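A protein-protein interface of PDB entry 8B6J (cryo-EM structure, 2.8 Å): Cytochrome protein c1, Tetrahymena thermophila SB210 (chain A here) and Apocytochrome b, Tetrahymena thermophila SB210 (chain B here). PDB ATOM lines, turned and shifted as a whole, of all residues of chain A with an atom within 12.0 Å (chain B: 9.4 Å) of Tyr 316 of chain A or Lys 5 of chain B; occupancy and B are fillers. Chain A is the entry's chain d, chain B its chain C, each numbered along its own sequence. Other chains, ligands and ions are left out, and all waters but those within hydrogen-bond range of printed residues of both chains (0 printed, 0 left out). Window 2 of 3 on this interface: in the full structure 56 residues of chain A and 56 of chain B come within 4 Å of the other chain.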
ATOM      1  N   ASN A 307      -0.242 -31.125 -16.377  1.00  0.00           N
ATOM      2  CA  ASN A 307      -0.883 -31.412 -17.653  1.00  0.00           C
ATOM      3  C   ASN A 307      -1.361 -30.106 -18.267  1.00  0.00           C
ATOM      4  O   ASN A 307      -2.018 -29.306 -17.595  1.00  0.00           O
ATOM      5  CB  ASN A 307      -2.053 -32.382 -17.479  1.00  0.00           C
ATOM      6  CG  ASN A 307      -2.490 -33.005 -18.785  1.00  0.00           C
ATOM      7  OD1 ASN A 307      -3.362 -32.481 -19.475  1.00  0.00           O
ATOM      8  ND2 ASN A 307      -1.885 -34.132 -19.134  1.00  0.00           N
ATOM      9  N   SER A 308      -1.035 -29.895 -19.544  1.00  0.00           N
ATOM     10  CA  SER A 308      -1.408 -28.648 -20.202  1.00  0.00           C
ATOM     11  C   SER A 308      -2.920 -28.484 -20.266  1.00  0.00           C
ATOM     12  O   SER A 308      -3.444 -27.392 -20.015  1.00  0.00           O
ATOM     13  CB  SER A 308      -0.809 -28.600 -21.607  1.00  0.00           C
ATOM     14  OG  SER A 308       0.603 -28.667 -21.560  1.00  0.00           O
ATOM     15  N   ARG A 309      -3.638 -29.554 -20.599  1.00  0.00           N
ATOM     16  CA  ARG A 309      -5.082 -29.509 -20.774  1.00  0.00           C
ATOM     17  C   ARG A 309      -5.840 -29.799 -19.485  1.00  0.00           C
ATOM     18  O   ARG A 309      -6.990 -30.249 -19.543  1.00  0.00           O
ATOM     19  CB  ARG A 309      -5.511 -30.493 -21.862  1.00  0.00           C
ATOM     20  CG  ARG A 309      -4.922 -30.195 -23.225  1.00  0.00           C
ATOM     21  CD  ARG A 309      -5.458 -31.140 -24.281  1.00  0.00           C
ATOM     22  NE  ARG A 309      -4.862 -30.888 -25.587  1.00  0.00           N
ATOM     23  CZ  ARG A 309      -5.289 -29.971 -26.444  1.00  0.00           C
ATOM     24  NH1 ARG A 309      -6.321 -29.190 -26.166  1.00  0.00           N
ATOM     25  NH2 ARG A 309      -4.667 -29.833 -27.611  1.00  0.00           N
ATOM     26  N   ALA A 310      -5.225 -29.553 -18.326  1.00  0.00           N
ATOM     27  CA  ALA A 310      -5.913 -29.806 -17.066  1.00  0.00           C
ATOM     28  C   ALA A 310      -7.205 -29.008 -16.967  1.00  0.00           C
ATOM     29  O   ALA A 310      -8.176 -29.473 -16.360  1.00  0.00           O
ATOM     30  CB  ALA A 310      -4.998 -29.473 -15.891  1.00  0.00           C
ATOM     31  N   TYR A 311      -7.240 -27.810 -17.552  1.00  0.00           N
ATOM     32  CA  TYR A 311      -8.459 -27.012 -17.509  1.00  0.00           C
ATOM     33  C   TYR A 311      -9.590 -27.685 -18.271  1.00  0.00           C
ATOM     34  O   TYR A 311     -10.766 -27.456 -17.966  1.00  0.00           O
ATOM     35  CB  TYR A 311      -8.195 -25.613 -18.068  1.00  0.00           C
ATOM     36  CG  TYR A 311      -7.994 -25.563 -19.564  1.00  0.00           C
ATOM     37  CD1 TYR A 311      -6.746 -25.785 -20.125  1.00  0.00           C
ATOM     38  CD2 TYR A 311      -9.052 -25.280 -20.415  1.00  0.00           C
ATOM     39  CE1 TYR A 311      -6.559 -25.734 -21.491  1.00  0.00           C
ATOM     40  CE2 TYR A 311      -8.875 -25.226 -21.781  1.00  0.00           C
ATOM     41  CZ  TYR A 311      -7.627 -25.454 -22.314  1.00  0.00           C
ATOM     42  OH  TYR A 311      -7.448 -25.403 -23.675  1.00  0.00           O
ATOM     43  N   GLN A 312      -9.263 -28.513 -19.263  1.00  0.00           N
ATOM     44  CA  GLN A 312     -10.277 -29.266 -19.988  1.00  0.00           C
ATOM     45  C   GLN A 312     -10.726 -30.514 -19.243  1.00  0.00           C
ATOM     46  O   GLN A 312     -11.761 -31.086 -19.600  1.00  0.00           O
ATOM     47  CB  GLN A 312      -9.753 -29.662 -21.369  1.00  0.00           C
ATOM     48  CG  GLN A 312      -9.432 -28.486 -22.268  1.00  0.00           C
ATOM     49  CD  GLN A 312      -9.049 -28.915 -23.665  1.00  0.00           C
ATOM     50  OE1 GLN A 312      -8.970 -30.105 -23.961  1.00  0.00           O
ATOM     51  NE2 GLN A 312      -8.808 -27.945 -24.536  1.00  0.00           N
ATOM     52  N   PHE A 313      -9.982 -30.947 -18.228  1.00  0.00           N
ATOM     53  CA  PHE A 313     -10.359 -32.104 -17.430  1.00  0.00           C
ATOM     54  C   PHE A 313     -10.961 -31.725 -16.086  1.00  0.00           C
ATOM     55  O   PHE A 313     -11.783 -32.477 -15.554  1.00  0.00           O
ATOM     56  CB  PHE A 313      -9.142 -33.004 -17.184  1.00  0.00           C
ATOM     57  CG  PHE A 313      -8.399 -33.383 -18.435  1.00  0.00           C
ATOM     58  CD1 PHE A 313      -9.059 -33.513 -19.643  1.00  0.00           C
ATOM     59  CD2 PHE A 313      -7.035 -33.608 -18.399  1.00  0.00           C
ATOM     60  CE1 PHE A 313      -8.372 -33.859 -20.790  1.00  0.00           C
ATOM     61  CE2 PHE A 313      -6.345 -33.953 -19.542  1.00  0.00           C
ATOM     62  CZ  PHE A 313      -7.015 -34.079 -20.739  1.00  0.00           C
ATOM     63  N   ARG A 314     -10.576 -30.579 -15.529  1.00  0.00           N
ATOM     64  CA  ARG A 314     -11.058 -30.192 -14.212  1.00  0.00           C
ATOM     65  C   ARG A 314     -12.555 -29.915 -14.262  1.00  0.00           C
ATOM     66  O   ARG A 314     -13.031 -29.157 -15.112  1.00  0.00           O
ATOM     67  CB  ARG A 314     -10.307 -28.958 -13.710  1.00  0.00           C
ATOM     68  CG  ARG A 314     -10.516 -28.683 -12.231  1.00  0.00           C
ATOM     69  CD  ARG A 314      -9.945 -27.342 -11.803  1.00  0.00           C
ATOM     70  NE  ARG A 314      -8.501 -27.260 -11.986  1.00  0.00           N
ATOM     71  CZ  ARG A 314      -7.901 -26.729 -13.043  1.00  0.00           C
ATOM     72  NH1 ARG A 314      -8.590 -26.230 -14.055  1.00  0.00           N
ATOM     73  NH2 ARG A 314      -6.572 -26.694 -13.083  1.00  0.00           N
ATOM     74  N   GLY A 315     -13.297 -30.533 -13.347  1.00  0.00           N
ATOM     75  CA  GLY A 315     -14.728 -30.349 -13.269  1.00  0.00           C
ATOM     76  C   GLY A 315     -15.533 -31.125 -14.284  1.00  0.00           C
ATOM     77  O   GLY A 315     -16.761 -30.975 -14.320  1.00  0.00           O
ATOM     78  N   TYR A 316     -14.895 -31.949 -15.106  1.00  0.00           N
ATOM     79  CA  TYR A 316     -15.586 -32.686 -16.158  1.00  0.00           C
ATOM     80  C   TYR A 316     -15.376 -34.191 -16.085  1.00  0.00           C
ATOM     81  O   TYR A 316     -16.322 -34.945 -16.324  1.00  0.00           O
ATOM     82  CB  TYR A 316     -15.126 -32.172 -17.532  1.00  0.00           C
ATOM     83  CG  TYR A 316     -15.525 -30.744 -17.829  1.00  0.00           C
ATOM     84  CD1 TYR A 316     -16.780 -30.445 -18.337  1.00  0.00           C
ATOM     85  CD2 TYR A 316     -14.642 -29.697 -17.608  1.00  0.00           C
ATOM     86  CE1 TYR A 316     -17.148 -29.143 -18.611  1.00  0.00           C
ATOM     87  CE2 TYR A 316     -15.001 -28.392 -17.879  1.00  0.00           C
ATOM     88  CZ  TYR A 316     -16.255 -28.121 -18.380  1.00  0.00           C
ATOM     89  OH  TYR A 316     -16.618 -26.822 -18.653  1.00  0.00           O
ATOM     90  N   PHE A 317     -14.171 -34.648 -15.753  1.00  0.00           N
ATOM     91  CA  PHE A 317     -13.804 -36.052 -15.868  1.00  0.00           C
ATOM     92  C   PHE A 317     -13.436 -36.639 -14.513  1.00  0.00           C
ATOM     93  O   PHE A 317     -12.964 -35.935 -13.618  1.00  0.00           O
ATOM     94  CB  PHE A 317     -12.613 -36.243 -16.816  1.00  0.00           C
ATOM     95  CG  PHE A 317     -12.875 -35.820 -18.233  1.00  0.00           C
ATOM     96  CD1 PHE A 317     -14.159 -35.793 -18.747  1.00  0.00           C
ATOM     97  CD2 PHE A 317     -11.825 -35.459 -19.054  1.00  0.00           C
ATOM     98  CE1 PHE A 317     -14.386 -35.406 -20.050  1.00  0.00           C
ATOM     99  CE2 PHE A 317     -12.047 -35.073 -20.356  1.00  0.00           C
ATOM    100  CZ  PHE A 317     -13.329 -35.047 -20.855  1.00  0.00           C
ATOM    101  N   TRP A 318     -13.664 -37.946 -14.377  1.00  0.00           N
ATOM    102  CA  TRP A 318     -13.136 -38.748 -13.275  1.00  0.00           C
ATOM    103  C   TRP A 318     -13.512 -38.137 -11.921  1.00  0.00           C
ATOM    104  O   TRP A 318     -12.667 -37.719 -11.129  1.00  0.00           O
ATOM    105  CB  TRP A 318     -11.616 -38.910 -13.406  1.00  0.00           C
ATOM    106  CG  TRP A 318     -11.160 -39.162 -14.813  1.00  0.00           C
ATOM    107  CD1 TRP A 318     -11.559 -40.171 -15.639  1.00  0.00           C
ATOM    108  CD2 TRP A 318     -10.205 -38.393 -15.554  1.00  0.00           C
ATOM    109  NE1 TRP A 318     -10.919 -40.073 -16.849  1.00  0.00           N
ATOM    110  CE2 TRP A 318     -10.082 -38.990 -16.822  1.00  0.00           C
ATOM    111  CE3 TRP A 318      -9.446 -37.255 -15.268  1.00  0.00           C
ATOM    112  CZ2 TRP A 318      -9.229 -38.488 -17.802  1.00  0.00           C
ATOM    113  CZ3 TRP A 318      -8.603 -36.759 -16.241  1.00  0.00           C
ATOM    114  CH2 TRP A 318      -8.501 -37.375 -17.492  1.00  0.00           C
ATOM    115  N   ALA A 319     -14.817 -38.094 -11.686  1.00  0.00           N
ATOM    116  CA  ALA A 319     -15.349 -37.654 -10.404  1.00  0.00           C
ATOM    117  C   ALA A 319     -16.825 -38.005 -10.319  1.00  0.00           C
ATOM    118  O   ALA A 319     -17.420 -38.014  -9.243  1.00  0.00           O
ATOM    119  CB  ALA A 319     -15.142 -36.165 -10.220  1.00  0.00           C
ATOM    120  OXT ALA A 319     -17.456 -38.292 -11.335  1.00  0.00           O
ATOM    121  N   MET B   1     -19.943 -15.584 -21.578  1.00  0.00           N
ATOM    122  CA  MET B   1     -19.671 -16.970 -22.051  1.00  0.00           C
ATOM    123  C   MET B   1     -18.876 -17.746 -21.008  1.00  0.00           C
ATOM    124  O   MET B   1     -17.796 -18.259 -21.290  1.00  0.00           O
ATOM    125  CB  MET B   1     -18.919 -16.945 -23.383  1.00  0.00           C
ATOM    126  CG  MET B   1     -17.624 -16.153 -23.358  1.00  0.00           C
ATOM    127  SD  MET B   1     -16.962 -15.862 -25.008  1.00  0.00           S
ATOM    128  CE  MET B   1     -16.720 -17.538 -25.580  1.00  0.00           C
ATOM    129  N   GLU B   2     -19.427 -17.833 -19.797  1.00  0.00           N
ATOM    130  CA  GLU B   2     -18.757 -18.556 -18.722  1.00  0.00           C
ATOM    131  C   GLU B   2     -18.543 -20.023 -19.062  1.00  0.00           C
ATOM    132  O   GLU B   2     -17.637 -20.653 -18.505  1.00  0.00           O
ATOM    133  CB  GLU B   2     -19.564 -18.426 -17.427  1.00  0.00           C
ATOM    134  CG  GLU B   2     -21.012 -18.896 -17.521  1.00  0.00           C
ATOM    135  CD  GLU B   2     -21.169 -20.391 -17.330  1.00  0.00           C
ATOM    136  OE1 GLU B   2     -20.177 -21.058 -16.971  1.00  0.00           O
ATOM    137  OE2 GLU B   2     -22.291 -20.900 -17.534  1.00  0.00           O
ATOM    138  N   TRP B   3     -19.357 -20.582 -19.958  1.00  0.00           N
ATOM    139  CA  TRP B   3     -19.188 -21.974 -20.362  1.00  0.00           C
ATOM    140  C   TRP B   3     -17.858 -22.220 -21.066  1.00  0.00           C
ATOM    141  O   TRP B   3     -17.439 -23.377 -21.180  1.00  0.00           O
ATOM    142  CB  TRP B   3     -20.344 -22.410 -21.270  1.00  0.00           C
ATOM    143  CG  TRP B   3     -20.849 -21.334 -22.188  1.00  0.00           C
ATOM    144  CD1 TRP B   3     -21.934 -20.532 -21.989  1.00  0.00           C
ATOM    145  CD2 TRP B   3     -20.284 -20.937 -23.443  1.00  0.00           C
ATOM    146  NE1 TRP B   3     -22.081 -19.664 -23.040  1.00  0.00           N
ATOM    147  CE2 TRP B   3     -21.082 -19.892 -23.947  1.00  0.00           C
ATOM    148  CE3 TRP B   3     -19.184 -21.366 -24.190  1.00  0.00           C
ATOM    149  CZ2 TRP B   3     -20.814 -19.271 -25.162  1.00  0.00           C
ATOM    150  CZ3 TRP B   3     -18.922 -20.747 -25.396  1.00  0.00           C
ATOM    151  CH2 TRP B   3     -19.732 -19.709 -25.868  1.00  0.00           C
ATOM    152  N   ASN B   4     -17.189 -21.173 -21.538  1.00  0.00           N
ATOM    153  CA  ASN B   4     -15.895 -21.295 -22.200  1.00  0.00           C
ATOM    154  C   ASN B   4     -14.781 -21.050 -21.191  1.00  0.00           C
ATOM    155  O   ASN B   4     -14.758 -20.006 -20.530  1.00  0.00           O
ATOM    156  CB  ASN B   4     -15.784 -20.306 -23.360  1.00  0.00           C
ATOM    157  CG  ASN B   4     -14.500 -20.467 -24.141  1.00  0.00           C
ATOM    158  OD1 ASN B   4     -13.439 -20.022 -23.711  1.00  0.00           O
ATOM    159  ND2 ASN B   4     -14.591 -21.101 -25.303  1.00  0.00           N
ATOM    160  N   LYS B   5     -13.863 -22.006 -21.077  1.00  0.00           N
ATOM    161  CA  LYS B   5     -12.798 -21.948 -20.085  1.00  0.00           C
ATOM    162  C   LYS B   5     -11.510 -21.327 -20.609  1.00  0.00           C
ATOM    163  O   LYS B   5     -10.555 -21.188 -19.837  1.00  0.00           O
ATOM    164  CB  LYS B   5     -12.503 -23.353 -19.550  1.00  0.00           C
ATOM    165  CG  LYS B   5     -13.086 -23.626 -18.174  1.00  0.00           C
ATOM    166  CD  LYS B   5     -14.597 -23.485 -18.167  1.00  0.00           C
ATOM    167  CE  LYS B   5     -15.176 -23.806 -16.802  1.00  0.00           C
ATOM    168  NZ  LYS B   5     -16.655 -23.639 -16.773  1.00  0.00           N
ATOM    169  N   GLY B   6     -11.447 -20.957 -21.887  1.00  0.00           N
ATOM    170  CA  GLY B   6     -10.287 -20.297 -22.441  1.00  0.00           C
ATOM    171  C   GLY B   6      -9.781 -21.025 -23.663  1.00  0.00           C
ATOM    172  O   GLY B   6     -10.524 -21.750 -24.332  1.00  0.00           O
ATOM    173  N   THR B   7      -8.496 -20.827 -23.953  1.00  0.00           N
ATOM    174  CA  THR B   7      -7.850 -21.405 -25.123  1.00  0.00           C
ATOM    175  C   THR B   7      -6.601 -22.160 -24.696  1.00  0.00           C
ATOM    176  O   THR B   7      -5.974 -21.835 -23.684  1.00  0.00           O
ATOM    177  CB  THR B   7      -7.476 -20.330 -26.149  1.00  0.00           C
ATOM    178  OG1 THR B   7      -6.595 -19.375 -25.546  1.00  0.00           O
ATOM    179  CG2 THR B   7      -8.718 -19.619 -26.651  1.00  0.00           C
ATOM    180  N   TYR B   8      -6.244 -23.175 -25.484  1.00  0.00           N
ATOM    181  CA  TYR B   8      -5.112 -24.026 -25.133  1.00  0.00           C
ATOM    182  C   TYR B   8      -3.809 -23.236 -25.112  1.00  0.00           C
ATOM    183  O   TYR B   8      -3.064 -23.270 -24.126  1.00  0.00           O
ATOM    184  CB  TYR B   8      -5.019 -25.196 -26.113  1.00  0.00           C
ATOM    185  CG  TYR B   8      -3.866 -26.134 -25.848  1.00  0.00           C
ATOM    186  CD1 TYR B   8      -3.904 -27.033 -24.794  1.00  0.00           C
ATOM    187  CD2 TYR B   8      -2.742 -26.126 -26.661  1.00  0.00           C
ATOM    188  CE1 TYR B   8      -2.855 -27.891 -24.550  1.00  0.00           C
ATOM    189  CE2 TYR B   8      -1.688 -26.982 -26.426  1.00  0.00           C
ATOM    190  CZ  TYR B   8      -1.748 -27.863 -25.370  1.00  0.00           C
ATOM    191  OH  TYR B   8      -0.698 -28.719 -25.133  1.00  0.00           O
ATOM    192  N   ASN B 319     -13.841 -42.023 -22.905  1.00  0.00           N
ATOM    193  CA  ASN B 319     -14.373 -40.764 -22.407  1.00  0.00           C
ATOM    194  C   ASN B 319     -14.224 -40.745 -20.889  1.00  0.00           C
ATOM    195  O   ASN B 319     -13.447 -41.512 -20.312  1.00  0.00           O
ATOM    196  CB  ASN B 319     -15.830 -40.593 -22.857  1.00  0.00           C
ATOM    197  CG  ASN B 319     -16.716 -41.722 -22.382  1.00  0.00           C
ATOM    198  OD1 ASN B 319     -16.234 -42.796 -22.028  1.00  0.00           O
ATOM    199  ND2 ASN B 319     -18.022 -41.486 -22.375  1.00  0.00           N
ATOM    200  N   GLU B 320     -14.962 -39.838 -20.246  1.00  0.00           N
ATOM    201  CA  GLU B 320     -14.993 -39.725 -18.793  1.00  0.00           C
ATOM    202  C   GLU B 320     -15.021 -41.097 -18.131  1.00  0.00           C
ATOM    203  O   GLU B 320     -14.344 -41.320 -17.122  1.00  0.00           O
ATOM    204  CB  GLU B 320     -16.215 -38.907 -18.363  1.00  0.00           C
ATOM    205  CG  GLU B 320     -16.475 -38.886 -16.864  1.00  0.00           C
ATOM    206  CD  GLU B 320     -17.707 -38.080 -16.498  1.00  0.00           C
ATOM    207  OE1 GLU B 320     -18.531 -37.812 -17.397  1.00  0.00           O
ATOM    208  OE2 GLU B 320     -17.851 -37.714 -15.313  1.00  0.00           O
ATOM    209  N   GLN B 321     -15.800 -42.017 -18.689  1.00  0.00           N
ATOM    210  CA  GLN B 321     -15.898 -43.367 -18.152  1.00  0.00           C
ATOM    211  C   GLN B 321     -14.757 -44.205 -18.716  1.00  0.00           C
ATOM    212  O   GLN B 321     -14.612 -44.324 -19.937  1.00  0.00           O
ATOM    213  CB  GLN B 321     -17.251 -43.980 -18.503  1.00  0.00           C
ATOM    214  CG  GLN B 321     -18.412 -43.001 -18.416  1.00  0.00           C
ATOM    215  CD  GLN B 321     -19.753 -43.655 -18.680  1.00  0.00           C
ATOM    216  OE1 GLN B 321     -20.169 -44.556 -17.953  1.00  0.00           O
ATOM    217  NE2 GLN B 321     -20.435 -43.206 -19.726  1.00  0.00           N
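Hydrophobic or aromatic side chains of chain A that line the printed part of chain B: Tyr 311, Tyr 316, Phe 317 and Trp 318.
Among the printed residues, 8 pairs touch across the chains.
Among the printed residues, no Asp or Glu carboxylate lies within 4 Å of a Lys or Arg side-chain nitrogen of the other chain.
Tyr 8 of chain B touches Ser 308 of chain A (OH to CB, 3.5 Å).
CG of Arg 309 of chain A touches CE1 of Tyr 8 of chain B, 3.4 Å away.
Tyr 311 of chain A touches Thr 7 of chain B (OH to C, 3.5 Å).
OH of Tyr 316 of chain A touches NZ of Lys 5 of chain B, 3.7 Å away.
CB of Glu 320 of chain B touches CD1 of Phe 317 of chain A, at 3.8 Å.
Glu 320 of chain B touches Trp 318 of chain A.
Asn 307 of chain A touches none of the printed residues of chain B.
Of the printed residues of chain B, Arg 309 of chain A touches Tyr 8.
Of the printed residues of chain B, Tyr 311 of chain A touches Thr 7 (3.5 Å) and Tyr 8 (3.1 Å).
Tyr 316 of chain A touches two residues of chain B.
Phe 317 of chain A touches just one residue of chain B: Glu 320.
Of the printed residues of chain B, Trp 318 of chain A touches Glu 320.
No residue of chain A comes within 4 Å of Asn 4 of chain B.
Lys 5 of chain B touches one residue of chain A.
No residue of chain A comes within 4 Å of Gly 6 of chain B.
Of chain A, only Tyr 311 comes within 4 Å of Thr 7 of chain B.
Of chain A, only Tyr 316 (3.3 Å), Phe 317 (3.8 Å) and Trp 318 (3.4 Å) come within 4 Å of Glu 320 of chain B.
The nearest printed residue of chain B that does not touch Arg 309 of chain A is Thr 7 of chain B (7.2 Å).
NE2 of Gln 312 of chain A is in hydrogen-bond range of OH of Tyr 311 of chain A.
NH1 of Arg 309 of chain A lies close to NE2 of Gln 312 of chain A, at 3.2 Å.
OD1 of Asn 307 of chain A lies within hydrogen-bond range of N of Arg 309 of chain A (3.1 Å).
The backbone NH of Tyr 8 of chain B sits close to the side-chain hydroxyl of Tyr 311 of chain A (3.1 Å).
The side-chain carboxylate (OE2) of Glu 320 of chain B sits close to the backbone carbonyl oxygen (O) of Tyr 316 of chain A (3.3 Å).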
